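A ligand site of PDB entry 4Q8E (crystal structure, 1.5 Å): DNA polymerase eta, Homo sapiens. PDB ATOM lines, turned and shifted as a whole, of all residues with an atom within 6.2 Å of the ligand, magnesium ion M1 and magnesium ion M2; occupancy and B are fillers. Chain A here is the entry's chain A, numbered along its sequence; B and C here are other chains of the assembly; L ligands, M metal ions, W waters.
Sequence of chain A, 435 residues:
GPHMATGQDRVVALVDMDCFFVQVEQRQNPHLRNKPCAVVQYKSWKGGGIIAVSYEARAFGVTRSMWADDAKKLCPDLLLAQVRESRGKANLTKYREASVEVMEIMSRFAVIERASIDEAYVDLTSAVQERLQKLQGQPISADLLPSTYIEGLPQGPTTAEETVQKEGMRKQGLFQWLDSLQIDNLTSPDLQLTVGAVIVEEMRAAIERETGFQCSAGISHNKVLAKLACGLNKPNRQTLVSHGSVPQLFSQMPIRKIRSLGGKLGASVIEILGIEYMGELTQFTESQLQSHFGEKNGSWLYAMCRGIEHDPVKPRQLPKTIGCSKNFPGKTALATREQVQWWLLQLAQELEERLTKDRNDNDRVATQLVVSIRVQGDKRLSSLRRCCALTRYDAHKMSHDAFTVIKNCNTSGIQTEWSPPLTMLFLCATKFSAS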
ATOM      1  N   ASP A  16       1.852  -1.932  26.480  1.00  0.00           N
ATOM      2  CA  ASP A  16       2.887  -1.226  25.730  1.00  0.00           C
ATOM      3  C   ASP A  16       4.014  -0.809  26.671  1.00  0.00           C
ATOM      4  O   ASP A  16       3.794  -0.090  27.648  1.00  0.00           O
ATOM      5  CB  ASP A  16       2.340   0.006  25.012  1.00  0.00           C
ATOM      6  CG  ASP A  16       3.400   0.647  24.145  1.00  0.00           C
ATOM      7  OD1 ASP A  16       4.223   1.337  24.699  1.00  0.00           O
ATOM      8  OD2 ASP A  16       3.455   0.377  22.937  1.00  0.00           O
ATOM      9  N   MET A  17       5.239  -1.184  26.337  1.00  0.00           N
ATOM     10  CA  MET A  17       6.340  -0.880  27.243  1.00  0.00           C
ATOM     11  C   MET A  17       6.611   0.610  27.307  1.00  0.00           C
ATOM     12  O   MET A  17       6.509   1.304  26.325  1.00  0.00           O
ATOM     13  CB  MET A  17       7.611  -1.603  26.766  1.00  0.00           C
ATOM     14  CG  MET A  17       7.423  -3.132  26.644  1.00  0.00           C
ATOM     15  SD  MET A  17       6.762  -3.974  28.098  1.00  0.00           S
ATOM     16  CE  MET A  17       8.054  -3.736  29.238  1.00  0.00           C
ATOM     17  N   ASP A  18       6.933   1.101  28.501  1.00  0.00           N
ATOM     18  CA  ASP A  18       7.289   2.523  28.625  1.00  0.00           C
ATOM     19  C   ASP A  18       8.694   2.762  28.103  1.00  0.00           C
ATOM     20  O   ASP A  18       9.610   1.937  28.348  1.00  0.00           O
ATOM     21  CB  ASP A  18       7.188   2.949  30.094  1.00  0.00           C
ATOM     22  CG  ASP A  18       5.767   2.819  30.645  1.00  0.00           C
ATOM     23  OD1 ASP A  18       4.816   2.932  29.852  1.00  0.00           O
ATOM     24  OD2 ASP A  18       5.609   2.631  31.853  1.00  0.00           O
ATOM     25  N   CYS A  19       8.877   3.876  27.388  1.00  0.00           N
ATOM     26  CA  CYS A  19      10.179   4.270  26.776  1.00  0.00           C
ATOM     27  C   CYS A  19      11.111   3.070  26.558  1.00  0.00           C
ATOM     28  O   CYS A  19      12.174   2.965  27.181  1.00  0.00           O
ATOM     29  CB  CYS A  19      10.854   5.416  27.553  1.00  0.00           C
ATOM     30  SG  CYS A  19      11.123   5.159  29.332  1.00  0.00           S
ATOM     31  N   PHE A  20      10.670   2.156  25.720  1.00  0.00           N
ATOM     32  CA  PHE A  20      11.203   0.785  25.785  1.00  0.00           C
ATOM     33  C   PHE A  20      12.716   0.705  25.606  1.00  0.00           C
ATOM     34  O   PHE A  20      13.371   0.134  26.450  1.00  0.00           O
ATOM     35  CB  PHE A  20      10.525  -0.116  24.753  1.00  0.00           C
ATOM     36  CG  PHE A  20      10.962  -1.559  24.813  1.00  0.00           C
ATOM     37  CD1 PHE A  20      11.014  -2.247  26.036  1.00  0.00           C
ATOM     38  CD2 PHE A  20      11.305  -2.230  23.654  1.00  0.00           C
ATOM     39  CE1 PHE A  20      11.411  -3.600  26.068  1.00  0.00           C
ATOM     40  CE2 PHE A  20      11.696  -3.604  23.692  1.00  0.00           C
ATOM     41  CZ  PHE A  20      11.741  -4.247  24.896  1.00  0.00           C
ATOM     42  N   PHE A  21      13.260   1.254  24.526  1.00  0.00           N
ATOM     43  CA  PHE A  21      14.701   1.047  24.290  1.00  0.00           C
ATOM     44  C   PHE A  21      15.507   1.721  25.402  1.00  0.00           C
ATOM     45  O   PHE A  21      16.574   1.260  25.765  1.00  0.00           O
ATOM     46  CB  PHE A  21      15.169   1.616  22.941  1.00  0.00           C
ATOM     47  CG  PHE A  21      14.715   0.845  21.724  1.00  0.00           C
ATOM     48  CD1 PHE A  21      13.739  -0.145  21.799  1.00  0.00           C
ATOM     49  CD2 PHE A  21      15.296   1.110  20.493  1.00  0.00           C
ATOM     50  CE1 PHE A  21      13.332  -0.836  20.632  1.00  0.00           C
ATOM     51  CE2 PHE A  21      14.894   0.416  19.339  1.00  0.00           C
ATOM     52  CZ  PHE A  21      13.889  -0.541  19.418  1.00  0.00           C
ATOM     53  N   VAL A  22      15.002   2.841  25.939  1.00  0.00           N
ATOM     54  CA  VAL A  22      15.650   3.484  27.080  1.00  0.00           C
ATOM     55  C   VAL A  22      15.640   2.528  28.299  1.00  0.00           C
ATOM     56  O   VAL A  22      16.655   2.378  28.972  1.00  0.00           O
ATOM     57  CB  VAL A  22      14.952   4.826  27.422  1.00  0.00           C
ATOM     58  CG1 VAL A  22      15.333   5.296  28.845  1.00  0.00           C
ATOM     59  CG2 VAL A  22      15.299   5.866  26.374  1.00  0.00           C
ATOM     60  N   GLN A  41      20.873   6.588  17.289  1.00  0.00           N
ATOM     61  CA  GLN A  41      21.479   5.822  16.195  1.00  0.00           C
ATOM     62  C   GLN A  41      22.443   6.729  15.429  1.00  0.00           C
ATOM     63  O   GLN A  41      22.066   7.840  15.060  1.00  0.00           O
ATOM     64  CB  GLN A  41      20.418   5.313  15.215  1.00  0.00           C
ATOM     65  CG  GLN A  41      19.428   4.310  15.762  1.00  0.00           C
ATOM     66  CD  GLN A  41      18.563   3.669  14.674  1.00  0.00           C
ATOM     67  OE1 GLN A  41      18.478   2.438  14.598  1.00  0.00           O
ATOM     68  NE2 GLN A  41      17.921   4.491  13.844  1.00  0.00           N
ATOM     69  N   ILE A  51      15.869   7.940  18.968  1.00  0.00           N
ATOM     70  CA  ILE A  51      14.744   7.064  18.669  1.00  0.00           C
ATOM     71  C   ILE A  51      13.899   6.702  19.898  1.00  0.00           C
ATOM     72  O   ILE A  51      12.824   6.132  19.755  1.00  0.00           O
ATOM     73  CB  ILE A  51      15.177   5.795  17.899  1.00  0.00           C
ATOM     74  CG1 ILE A  51      16.126   4.886  18.714  1.00  0.00           C
ATOM     75  CG2 ILE A  51      15.831   6.230  16.578  1.00  0.00           C
ATOM     76  CD1 ILE A  51      16.365   3.531  18.017  1.00  0.00           C
ATOM     77  N   ALA A  52      14.375   7.025  21.103  1.00  0.00           N
ATOM     78  CA  ALA A  52      13.612   6.787  22.338  1.00  0.00           C
ATOM     79  C   ALA A  52      14.098   7.731  23.404  1.00  0.00           C
ATOM     80  O   ALA A  52      15.280   8.099  23.415  1.00  0.00           O
ATOM     81  CB  ALA A  52      13.722   5.320  22.804  1.00  0.00           C
ATOM     82  N   VAL A  53      13.189   8.130  24.296  1.00  0.00           N
ATOM     83  CA  VAL A  53      13.416   9.228  25.253  1.00  0.00           C
ATOM     84  C   VAL A  53      12.792   8.908  26.600  1.00  0.00           C
ATOM     85  O   VAL A  53      11.593   8.579  26.675  1.00  0.00           O
ATOM     86  CB  VAL A  53      12.803  10.560  24.715  1.00  0.00           C
ATOM     87  CG1 VAL A  53      13.251  11.727  25.553  1.00  0.00           C
ATOM     88  CG2 VAL A  53      13.217  10.823  23.274  1.00  0.00           C
ATOM     89  N   TYR A  55      11.192   9.572  30.310  1.00  0.00           N
ATOM     90  CA  TYR A  55      10.206  10.554  30.718  1.00  0.00           C
ATOM     91  C   TYR A  55      10.866  11.772  31.368  1.00  0.00           C
ATOM     92  O   TYR A  55      10.364  12.891  31.209  1.00  0.00           O
ATOM     93  CB  TYR A  55       9.131   9.932  31.603  1.00  0.00           C
ATOM     94  CG  TYR A  55       8.146   9.150  30.764  1.00  0.00           C
ATOM     95  CD1 TYR A  55       8.441   7.854  30.304  1.00  0.00           C
ATOM     96  CD2 TYR A  55       6.978   9.735  30.319  1.00  0.00           C
ATOM     97  CE1 TYR A  55       7.572   7.174  29.459  1.00  0.00           C
ATOM     98  CE2 TYR A  55       6.101   9.053  29.493  1.00  0.00           C
ATOM     99  CZ  TYR A  55       6.387   7.773  29.064  1.00  0.00           C
ATOM    100  OH  TYR A  55       5.515   7.101  28.230  1.00  0.00           O
ATOM    101  N   ARG A  58      11.805  13.858  28.459  1.00  0.00           N
ATOM    102  CA  ARG A  58      10.636  14.437  27.796  1.00  0.00           C
ATOM    103  C   ARG A  58      10.159  15.727  28.463  1.00  0.00           C
ATOM    104  O   ARG A  58       9.633  16.607  27.775  1.00  0.00           O
ATOM    105  CB  ARG A  58       9.471  13.449  27.717  1.00  0.00           C
ATOM    106  CG  ARG A  58       9.754  12.244  26.882  1.00  0.00           C
ATOM    107  CD  ARG A  58       8.589  11.287  26.927  1.00  0.00           C
ATOM    108  NE  ARG A  58       9.003   9.939  26.532  1.00  0.00           N
ATOM    109  CZ  ARG A  58       8.218   8.953  26.153  1.00  0.00           C
ATOM    110  NH1 ARG A  58       6.911   9.122  26.036  1.00  0.00           N
ATOM    111  NH2 ARG A  58       8.778   7.772  25.838  1.00  0.00           N
ATOM    112  N   ARG A  64      11.636  11.977  20.136  1.00  0.00           N
ATOM    113  CA  ARG A  64      12.022  11.157  18.999  1.00  0.00           C
ATOM    114  C   ARG A  64      12.199  12.004  17.727  1.00  0.00           C
ATOM    115  O   ARG A  64      11.529  13.021  17.540  1.00  0.00           O
ATOM    116  CB  ARG A  64      10.921  10.094  18.839  1.00  0.00           C
ATOM    117  CG  ARG A  64      10.828   9.460  17.450  1.00  0.00           C
ATOM    118  CD  ARG A  64       9.964   8.210  17.497  1.00  0.00           C
ATOM    119  NE  ARG A  64      10.355   7.402  18.638  1.00  0.00           N
ATOM    120  CZ  ARG A  64       9.520   6.898  19.539  1.00  0.00           C
ATOM    121  NH1 ARG A  64       8.209   7.067  19.431  1.00  0.00           N
ATOM    122  NH2 ARG A  64      10.013   6.203  20.551  1.00  0.00           N
ATOM    123  N   SER A 116       4.090  -5.028  17.883  1.00  0.00           N
ATOM    124  CA  SER A 116       5.296  -4.285  17.568  1.00  0.00           C
ATOM    125  C   SER A 116       6.380  -4.846  18.481  1.00  0.00           C
ATOM    126  O   SER A 116       6.127  -5.731  19.271  1.00  0.00           O
ATOM    127  CB  SER A 116       5.156  -2.801  17.843  1.00  0.00           C
ATOM    128  OG  SER A 116       5.245  -2.524  19.241  1.00  0.00           O
ATOM    129  N   ILE A 117       7.577  -4.291  18.390  1.00  0.00           N
ATOM    130  CA  ILE A 117       8.652  -4.742  19.259  1.00  0.00           C
ATOM    131  C   ILE A 117       8.308  -4.571  20.749  1.00  0.00           C
ATOM    132  O   ILE A 117       8.847  -5.283  21.582  1.00  0.00           O
ATOM    133  CB  ILE A 117       9.978  -4.034  18.902  1.00  0.00           C
ATOM    134  CG1 ILE A 117      11.177  -4.854  19.396  1.00  0.00           C
ATOM    135  CG2 ILE A 117      10.001  -2.606  19.433  1.00  0.00           C
ATOM    136  CD1 ILE A 117      12.486  -4.380  18.796  1.00  0.00           C
ATOM    137  N   ASP A 118       7.424  -3.627  21.075  1.00  0.00           N
ATOM    138  CA  ASP A 118       7.151  -3.391  22.494  1.00  0.00           C
ATOM    139  C   ASP A 118       5.690  -3.401  22.890  1.00  0.00           C
ATOM    140  O   ASP A 118       5.330  -2.942  23.984  1.00  0.00           O
ATOM    141  CB  ASP A 118       7.829  -2.094  22.964  1.00  0.00           C
ATOM    142  CG  ASP A 118       6.931  -0.896  22.792  1.00  0.00           C
ATOM    143  OD1 ASP A 118       6.162  -0.806  21.778  1.00  0.00           O
ATOM    144  OD2 ASP A 118       6.973  -0.050  23.707  1.00  0.00           O
ATOM    145  N   GLU A 119       4.851  -3.994  22.058  1.00  0.00           N
ATOM    146  CA  GLU A 119       3.480  -4.123  22.510  1.00  0.00           C
ATOM    147  C   GLU A 119       2.771  -5.323  21.962  1.00  0.00           C
ATOM    148  O   GLU A 119       3.161  -5.874  20.924  1.00  0.00           O
ATOM    149  CB  GLU A 119       2.695  -2.884  22.205  1.00  0.00           C
ATOM    150  CG  GLU A 119       2.461  -2.648  20.798  1.00  0.00           C
ATOM    151  CD  GLU A 119       2.386  -1.160  20.501  1.00  0.00           C
ATOM    152  OE1 GLU A 119       1.267  -0.640  20.374  1.00  0.00           O
ATOM    153  OE2 GLU A 119       3.450  -0.523  20.419  1.00  0.00           O
ATOM    154  N   LYS A 227      -5.982   0.204  22.838  1.00  0.00           N
ATOM    155  CA  LYS A 227      -4.784   0.966  22.467  1.00  0.00           C
ATOM    156  C   LYS A 227      -4.947   2.417  22.902  1.00  0.00           C
ATOM    157  O   LYS A 227      -4.013   2.985  23.455  1.00  0.00           O
ATOM    158  CB  LYS A 227      -4.552   0.893  20.943  1.00  0.00           C
ATOM    159  CG  LYS A 227      -3.392   1.733  20.424  1.00  0.00           C
ATOM    160  CD  LYS A 227      -2.054   1.389  21.110  1.00  0.00           C
ATOM    161  CE  LYS A 227      -0.869   2.038  20.371  1.00  0.00           C
ATOM    162  NZ  LYS A 227       0.425   1.922  21.121  1.00  0.00           N
ATOM    163  N   LYS A 234      -0.199   6.624  30.634  1.00  0.00           N
ATOM    164  CA  LYS A 234       1.210   6.277  30.532  1.00  0.00           C
ATOM    165  C   LYS A 234       2.056   7.375  31.189  1.00  0.00           C
ATOM    166  O   LYS A 234       1.745   8.575  30.988  1.00  0.00           O
ATOM    167  CB  LYS A 234       1.508   6.152  29.039  1.00  0.00           C
ATOM    168  CG  LYS A 234       2.657   5.275  28.646  1.00  0.00           C
ATOM    169  CD  LYS A 234       2.768   5.202  27.125  1.00  0.00           C
ATOM    170  CE  LYS A 234       2.811   3.737  26.661  1.00  0.00           C
ATOM    171  NZ  LYS A 234       4.012   3.000  27.209  1.00  0.00           N
ATOM    172  N   PRO A 235       3.129   7.035  31.940  1.00  0.00           N
ATOM    173  CA  PRO A 235       3.741   5.703  32.096  1.00  0.00           C
ATOM    174  C   PRO A 235       3.374   5.003  33.384  1.00  0.00           C
ATOM    175  O   PRO A 235       2.860   5.599  34.343  1.00  0.00           O
ATOM    176  CB  PRO A 235       5.247   6.024  32.148  1.00  0.00           C
ATOM    177  CG  PRO A 235       5.296   7.361  32.853  1.00  0.00           C
ATOM    178  CD  PRO A 235       4.009   8.082  32.517  1.00  0.00           C
ATOM    179  P    DG B   8       1.029   2.553  16.809  1.00  0.00           P
ATOM    180  OP1  DG B   8       0.160   1.404  16.550  1.00  0.00           O
ATOM    181  OP2  DG B   8       0.724   3.436  17.955  1.00  0.00           O
ATOM    182  O5'  DG B   8       2.563   2.131  16.912  1.00  0.00           O
ATOM    183  C5'  DG B   8       2.861   0.907  17.464  1.00  0.00           C
ATOM    184  C4'  DG B   8       4.360   0.679  17.457  1.00  0.00           C
ATOM    185  O4'  DG B   8       4.972   0.878  16.177  1.00  0.00           O
ATOM    186  C3'  DG B   8       5.226   1.461  18.432  1.00  0.00           C
ATOM    187  O3'  DG B   8       5.787   0.563  19.274  1.00  0.00           O
ATOM    188  C2'  DG B   8       6.338   2.078  17.617  1.00  0.00           C
ATOM    189  C1'  DG B   8       6.309   1.279  16.332  1.00  0.00           C
ATOM    190  N9   DG B   8       6.656   2.128  15.206  1.00  0.00           N
ATOM    191  C8   DG B   8       5.875   3.097  14.620  1.00  0.00           C
ATOM    192  N7   DG B   8       6.465   3.717  13.643  1.00  0.00           N
ATOM    193  C5   DG B   8       7.711   3.108  13.551  1.00  0.00           C
ATOM    194  C6   DG B   8       8.792   3.343  12.665  1.00  0.00           C
ATOM    195  O6   DG B   8       8.879   4.153  11.743  1.00  0.00           O
ATOM    196  N1   DG B   8       9.876   2.507  12.946  1.00  0.00           N
ATOM    197  C2   DG B   8       9.917   1.582  13.940  1.00  0.00           C
ATOM    198  N2   DG B   8      11.061   0.901  14.047  1.00  0.00           N
ATOM    199  N3   DG B   8       8.898   1.340  14.774  1.00  0.00           N
ATOM    200  C4   DG B   8       7.843   2.130  14.510  1.00  0.00           C
ATOM    201  O3' P9G C   2      19.042   4.572   9.243  1.00  0.00           O
ATOM    202  OP2 P9G C   2      18.281   9.003   6.636  1.00  0.00           O
ATOM    203  P   P9G C   2      17.040   9.330   7.404  1.00  0.00           P
ATOM    204  OP1 P9G C   2      15.715   8.928   6.862  1.00  0.00           O
ATOM    205  O5' P9G C   2      17.220   8.519   8.752  1.00  0.00           O
ATOM    206  C5' P9G C   2      18.528   8.188   9.241  1.00  0.00           C
ATOM    207  C4' P9G C   2      18.545   6.780   9.774  1.00  0.00           C
ATOM    208  O4' P9G C   2      17.486   6.621  10.744  1.00  0.00           O
ATOM    209  C1' P9G C   2      16.509   5.699  10.271  1.00  0.00           C
ATOM    210  C2' P9G C   2      16.794   5.512   8.788  1.00  0.00           C
ATOM    211  C3' P9G C   2      18.303   5.685   8.746  1.00  0.00           C
ATOM    212  N9  P9G C   2      15.207   6.209  10.688  1.00  0.00           N
ATOM    213  C8  P9G C   2      14.535   7.319  10.240  1.00  0.00           C
ATOM    214  N7  P9G C   2      13.429   7.539  10.899  1.00  0.00           N
ATOM    215  C5  P9G C   2      13.394   6.545  11.864  1.00  0.00           C
ATOM    216  C6  P9G C   2      12.459   6.284  12.893  1.00  0.00           C
ATOM    217  O6  P9G C   2      11.408   6.888  13.153  1.00  0.00           O
ATOM    218  N1  P9G C   2      12.831   5.181  13.665  1.00  0.00           N
ATOM    219  C2  P9G C   2      13.963   4.436  13.476  1.00  0.00           C
ATOM    220  N2  P9G C   2      14.154   3.409  14.323  1.00  0.00           N
ATOM    221  N3  P9G C   2      14.854   4.678  12.523  1.00  0.00           N
ATOM    222  C4  P9G C   2      14.512   5.735  11.770  1.00  0.00           C
ATOM    223 PT1  P9G C   2      12.074   9.048  10.576  1.00  0.00          PT
ATOM    224  N12 P9G C   2      10.658   7.673  10.129  1.00  0.00           N
ATOM    225  N11 P9G C   2      10.714  10.535  10.260  1.00  0.00           N
ATOM    226  N10 P9G C   2      13.483  10.443  11.023  1.00  0.00           N
ATOM    227  C18 P9G C   2      13.638  11.522  10.227  1.00  0.00           C
ATOM    228  C13 P9G C   2      14.590  12.474  10.529  1.00  0.00           C
ATOM    229  C12 P9G C   2      14.753  13.578   9.696  1.00  0.00           C
ATOM    230  C11 P9G C   2      15.705  14.540  10.000  1.00  0.00           C
ATOM    231  C10 P9G C   2      16.489  14.400  11.124  1.00  0.00           C
ATOM    232  C16 P9G C   2      14.250  10.303  12.162  1.00  0.00           C
ATOM    233  C22 P9G C   2      14.067   9.220  13.000  1.00  0.00           C
ATOM    234  C21 P9G C   2      14.881   9.058  14.122  1.00  0.00           C
ATOM    235  C20 P9G C   2      15.832  10.010  14.424  1.00  0.00           C
ATOM    236  C19 P9G C   2      16.004  11.113  13.595  1.00  0.00           C
ATOM    237  C15 P9G C   2      15.211  11.254  12.467  1.00  0.00           C
ATOM    238  C14 P9G C   2      15.375  12.344  11.655  1.00  0.00           C
ATOM    239  C9  P9G C   2      16.330  13.298  11.947  1.00  0.00           C
ATOM    240  P    DC C   3      19.194   3.203   8.432  1.00  0.00           P
ATOM    241  OP1  DC C   3      20.581   2.851   8.495  1.00  0.00           O
ATOM    242  OP2  DC C   3      18.477   3.352   7.141  1.00  0.00           O
ATOM    243  O5'  DC C   3      18.271   2.169   9.264  1.00  0.00           O
ATOM    244  C5'  DC C   3      18.648   1.778  10.604  1.00  0.00           C
ATOM    245  C4'  DC C   3      17.644   0.779  11.134  1.00  0.00           C
ATOM    246  O4'  DC C   3      16.431   1.522  11.387  1.00  0.00           O
ATOM    247  C3'  DC C   3      17.275  -0.358  10.190  1.00  0.00           C
ATOM    248  O3'  DC C   3      17.059  -1.534  10.993  1.00  0.00           O
ATOM    249  C2'  DC C   3      15.987   0.128   9.543  1.00  0.00           C
ATOM    250  C1'  DC C   3      15.374   0.810  10.788  1.00  0.00           C
ATOM    251  N1   DC C   3      14.270   1.738  10.510  1.00  0.00           N
ATOM    252  C2   DC C   3      13.187   1.768  11.394  1.00  0.00           C
ATOM    253  O2   DC C   3      13.185   1.013  12.369  1.00  0.00           O
ATOM    254  N3   DC C   3      12.158   2.596  11.134  1.00  0.00           N
ATOM    255  C4   DC C   3      12.189   3.412  10.081  1.00  0.00           C
ATOM    256  N4   DC C   3      11.140   4.224   9.866  1.00  0.00           N
ATOM    257  C5   DC C   3      13.300   3.401   9.189  1.00  0.00           C
ATOM    258  C6   DC C   3      14.310   2.566   9.440  1.00  0.00           C
HETATM  259  P1  LIG L   1       6.265   5.191  25.303  1.00  0.00           P
HETATM  260  O1  LIG L   1       5.616   6.478  24.810  1.00  0.00           O
HETATM  261  O2  LIG L   1       5.594   3.912  24.849  1.00  0.00           O
HETATM  262  O3  LIG L   1       6.395   5.195  26.794  1.00  0.00           O
HETATM  263  P2  LIG L   1       8.408   4.188  23.661  1.00  0.00           P
HETATM  264  O4  LIG L   1       9.883   4.556  23.563  1.00  0.00           O
HETATM  265  O5  LIG L   1       8.183   2.764  24.113  1.00  0.00           O
HETATM  266  O6  LIG L   1       7.725   5.219  24.668  1.00  0.00           O
HETATM  267  P3  LIG L   1       6.900   3.337  21.257  1.00  0.00           P
HETATM  268  O7  LIG L   1       5.992   2.467  22.007  1.00  0.00           O
HETATM  269  O8  LIG L   1       6.220   4.167  20.141  1.00  0.00           O
HETATM  270  N1  LIG L   1       7.628   4.539  22.226  1.00  0.00           N
HETATM  271  O9  LIG L   1       8.055   2.531  20.548  1.00  0.00           O
HETATM  272  C1  LIG L   1       8.751   1.480  21.122  1.00  0.00           C
HETATM  273  C2  LIG L   1      10.198   1.494  20.709  1.00  0.00           C
HETATM  274  O10 LIG L   1      10.247   1.340  19.284  1.00  0.00           O
HETATM  275  C3  LIG L   1      10.885   2.733  21.023  1.00  0.00           C
HETATM  276  O11 LIG L   1      11.439   2.703  22.359  1.00  0.00           O
HETATM  277  C4  LIG L   1      11.962   2.803  20.029  1.00  0.00           C
HETATM  278  C5  LIG L   1      11.309   2.180  18.823  1.00  0.00           C
HETATM  279  N2  LIG L   1      10.792   3.095  17.849  1.00  0.00           N
HETATM  280  C6  LIG L   1      11.645   3.440  16.785  1.00  0.00           C
HETATM  281  N3  LIG L   1      11.113   4.326  15.812  1.00  0.00           N
HETATM  282  C7  LIG L   1       9.871   4.827  15.937  1.00  0.00           C
HETATM  283  C8  LIG L   1       8.989   4.454  17.062  1.00  0.00           C
HETATM  284  C9  LIG L   1       9.469   3.569  18.003  1.00  0.00           C
HETATM  285  O12 LIG L   1      12.793   2.963  16.690  1.00  0.00           O
HETATM  286  N4  LIG L   1       9.421   5.721  14.923  1.00  0.00           N
HETATM  287 MG    MG M   1       6.183   1.908  24.195  1.00  0.00          MG
HETATM  288 MG    MG M   2       4.588   0.673  21.448  1.00  0.00          MG
HETATM  289  O   HOH W   1      13.997   0.659  16.036  1.00  0.00           O
HETATM  290  O   HOH W   2       3.256   4.181  23.174  1.00  0.00           O
HETATM  291  O   HOH W   3      10.576   7.190  23.669  1.00  0.00           O
HETATM  292  O   HOH W   4       9.821  -0.048  17.012  1.00  0.00           O
HETATM  293  O   HOH W   5       6.598   6.847  15.363  1.00  0.00           O
HETATM  294  O   HOH W   6       3.480   2.431  21.008  1.00  0.00           O
HETATM  295  O   HOH W   7       6.454   7.719  22.541  1.00  0.00           O
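Ser 116 touches magnesium ion M2 (OG to MG, 3.9 Å). Within 4 Å of magnesium ion M2: Asp 16, Ser 116, Asp 118, Glu 119 and DG 8 of chain B.
Magnesium ion M1 is bound by OD1 of Asp 16 (2.1 Å), OD2 of Asp 118 (2.2 Å), O5 of the ligand (2.2 Å), O2 of the ligand (2.2 Å), O of Met 17 (2.2 Å) and O7 of the ligand (2.3 Å).
Merely in contact with the ligand: Asp 18 (3.4 Å), Ile 51 (3.4 Å), Ala 52 (3.5 Å) and Ile 117 (3.96 Å). Of the 24 residues printed, 16 come within 4 Å of the ligand. Along chain A the residues within 4 Å of the ligand span positions 16 to 234.
O3' of DG 8 of chain B sits close to the side-chain hydroxyl (OG) of Ser 116 (3.1 Å). The guanidinium group of Arg 64 lies within hydrogen-bond range of the backbone carbonyl oxygen of Ile 51, at 2.9 Å. OH of Tyr 55 sits at hydrogen-bond distance from NH1 of Arg 58, at 3.3 Å. O2 of DC 3 of chain C lies close to N2 of DG 8 of chain B (2.7 Å). N3 of P9G 2 of chain C lies within hydrogen-bond range of the side-chain amide nitrogen (NE2) of Gln 41 (3.3 Å). The side-chain carboxylate (OD2) of Asp 16 sits close to the side-chain amino group (NZ) of Lys 227 (3.9 Å). The side-chain carboxylate (OE1) of Glu 119 lies within salt-bridge range of the side-chain amino group (NZ) of Lys 227 (2.8 Å). O of Asp 16 is in hydrogen-bond range of NZ of Lys 234, at 3.1 Å.
Lys 234 touches magnesium ion M1. Within 4 Å of magnesium ion M1: Asp 16, Met 17, Asp 118 and Lys 234. The nearest printed residue that does not touch magnesium ion M1 is Asp 18 (4.4 Å).
Water W6 lies within hydrogen-bond range of NZ of Lys 227 (3.1 Å) and O8 of the ligand (3.4 Å). Water W1 lies within hydrogen-bond range of an oxygen (O12) of the ligand (2.7 Å) and N2 of P9G 2 of chain C (3.2 Å). Water W4 lies within hydrogen-bond range of O10 of the ligand (2.7 Å) and N3 of DG 8 of chain B (2.8 Å).
Magnesium ion M2 is bound by OD2 of Asp 16. Magnesium ion M2 is bound by the side-chain carboxylate (OE2) of Glu 119 (1.9 Å). Water W6 binds magnesium ion M2 (2.1 Å). OD1 of Asp 118 is bound to magnesium ion M2. Magnesium ion M2 is bound by an oxygen (O7) of the ligand, at 2.3 Å. O3' of DG 8 of chain B is bound to magnesium ion M2 (2.5 Å). Magnesium ion M2 has six donor atoms within binding distance.
N of Phe 21 is in hydrogen-bond range of O11 of the ligand (3.2 Å). An oxygen (O4) of the ligand is in salt-bridge range of the guanidinium group of Arg 64, at 3.4 Å. An oxygen (O3) of the ligand lies within hydrogen-bond range of the side-chain hydroxyl (OH) of Tyr 55 (2.5 Å). The side-chain amino group (NZ) of Lys 234 is in salt-bridge range of an oxygen (O3) of the ligand, at 3.3 Å. O4 of the ligand lies within hydrogen-bond range of N of Phe 20, at 3.3 Å. The guanidinium group of Arg 58 is in salt-bridge range of an oxygen (O1) of the ligand (3.2 Å). The backbone NH (N) of Cys 19 sits at hydrogen-bond distance from an oxygen (O3) of the ligand, 2.9 Å away. A nitrogen (N4) of the ligand is in hydrogen-bond range of O6 of P9G 2 of chain C (2.9 Å).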
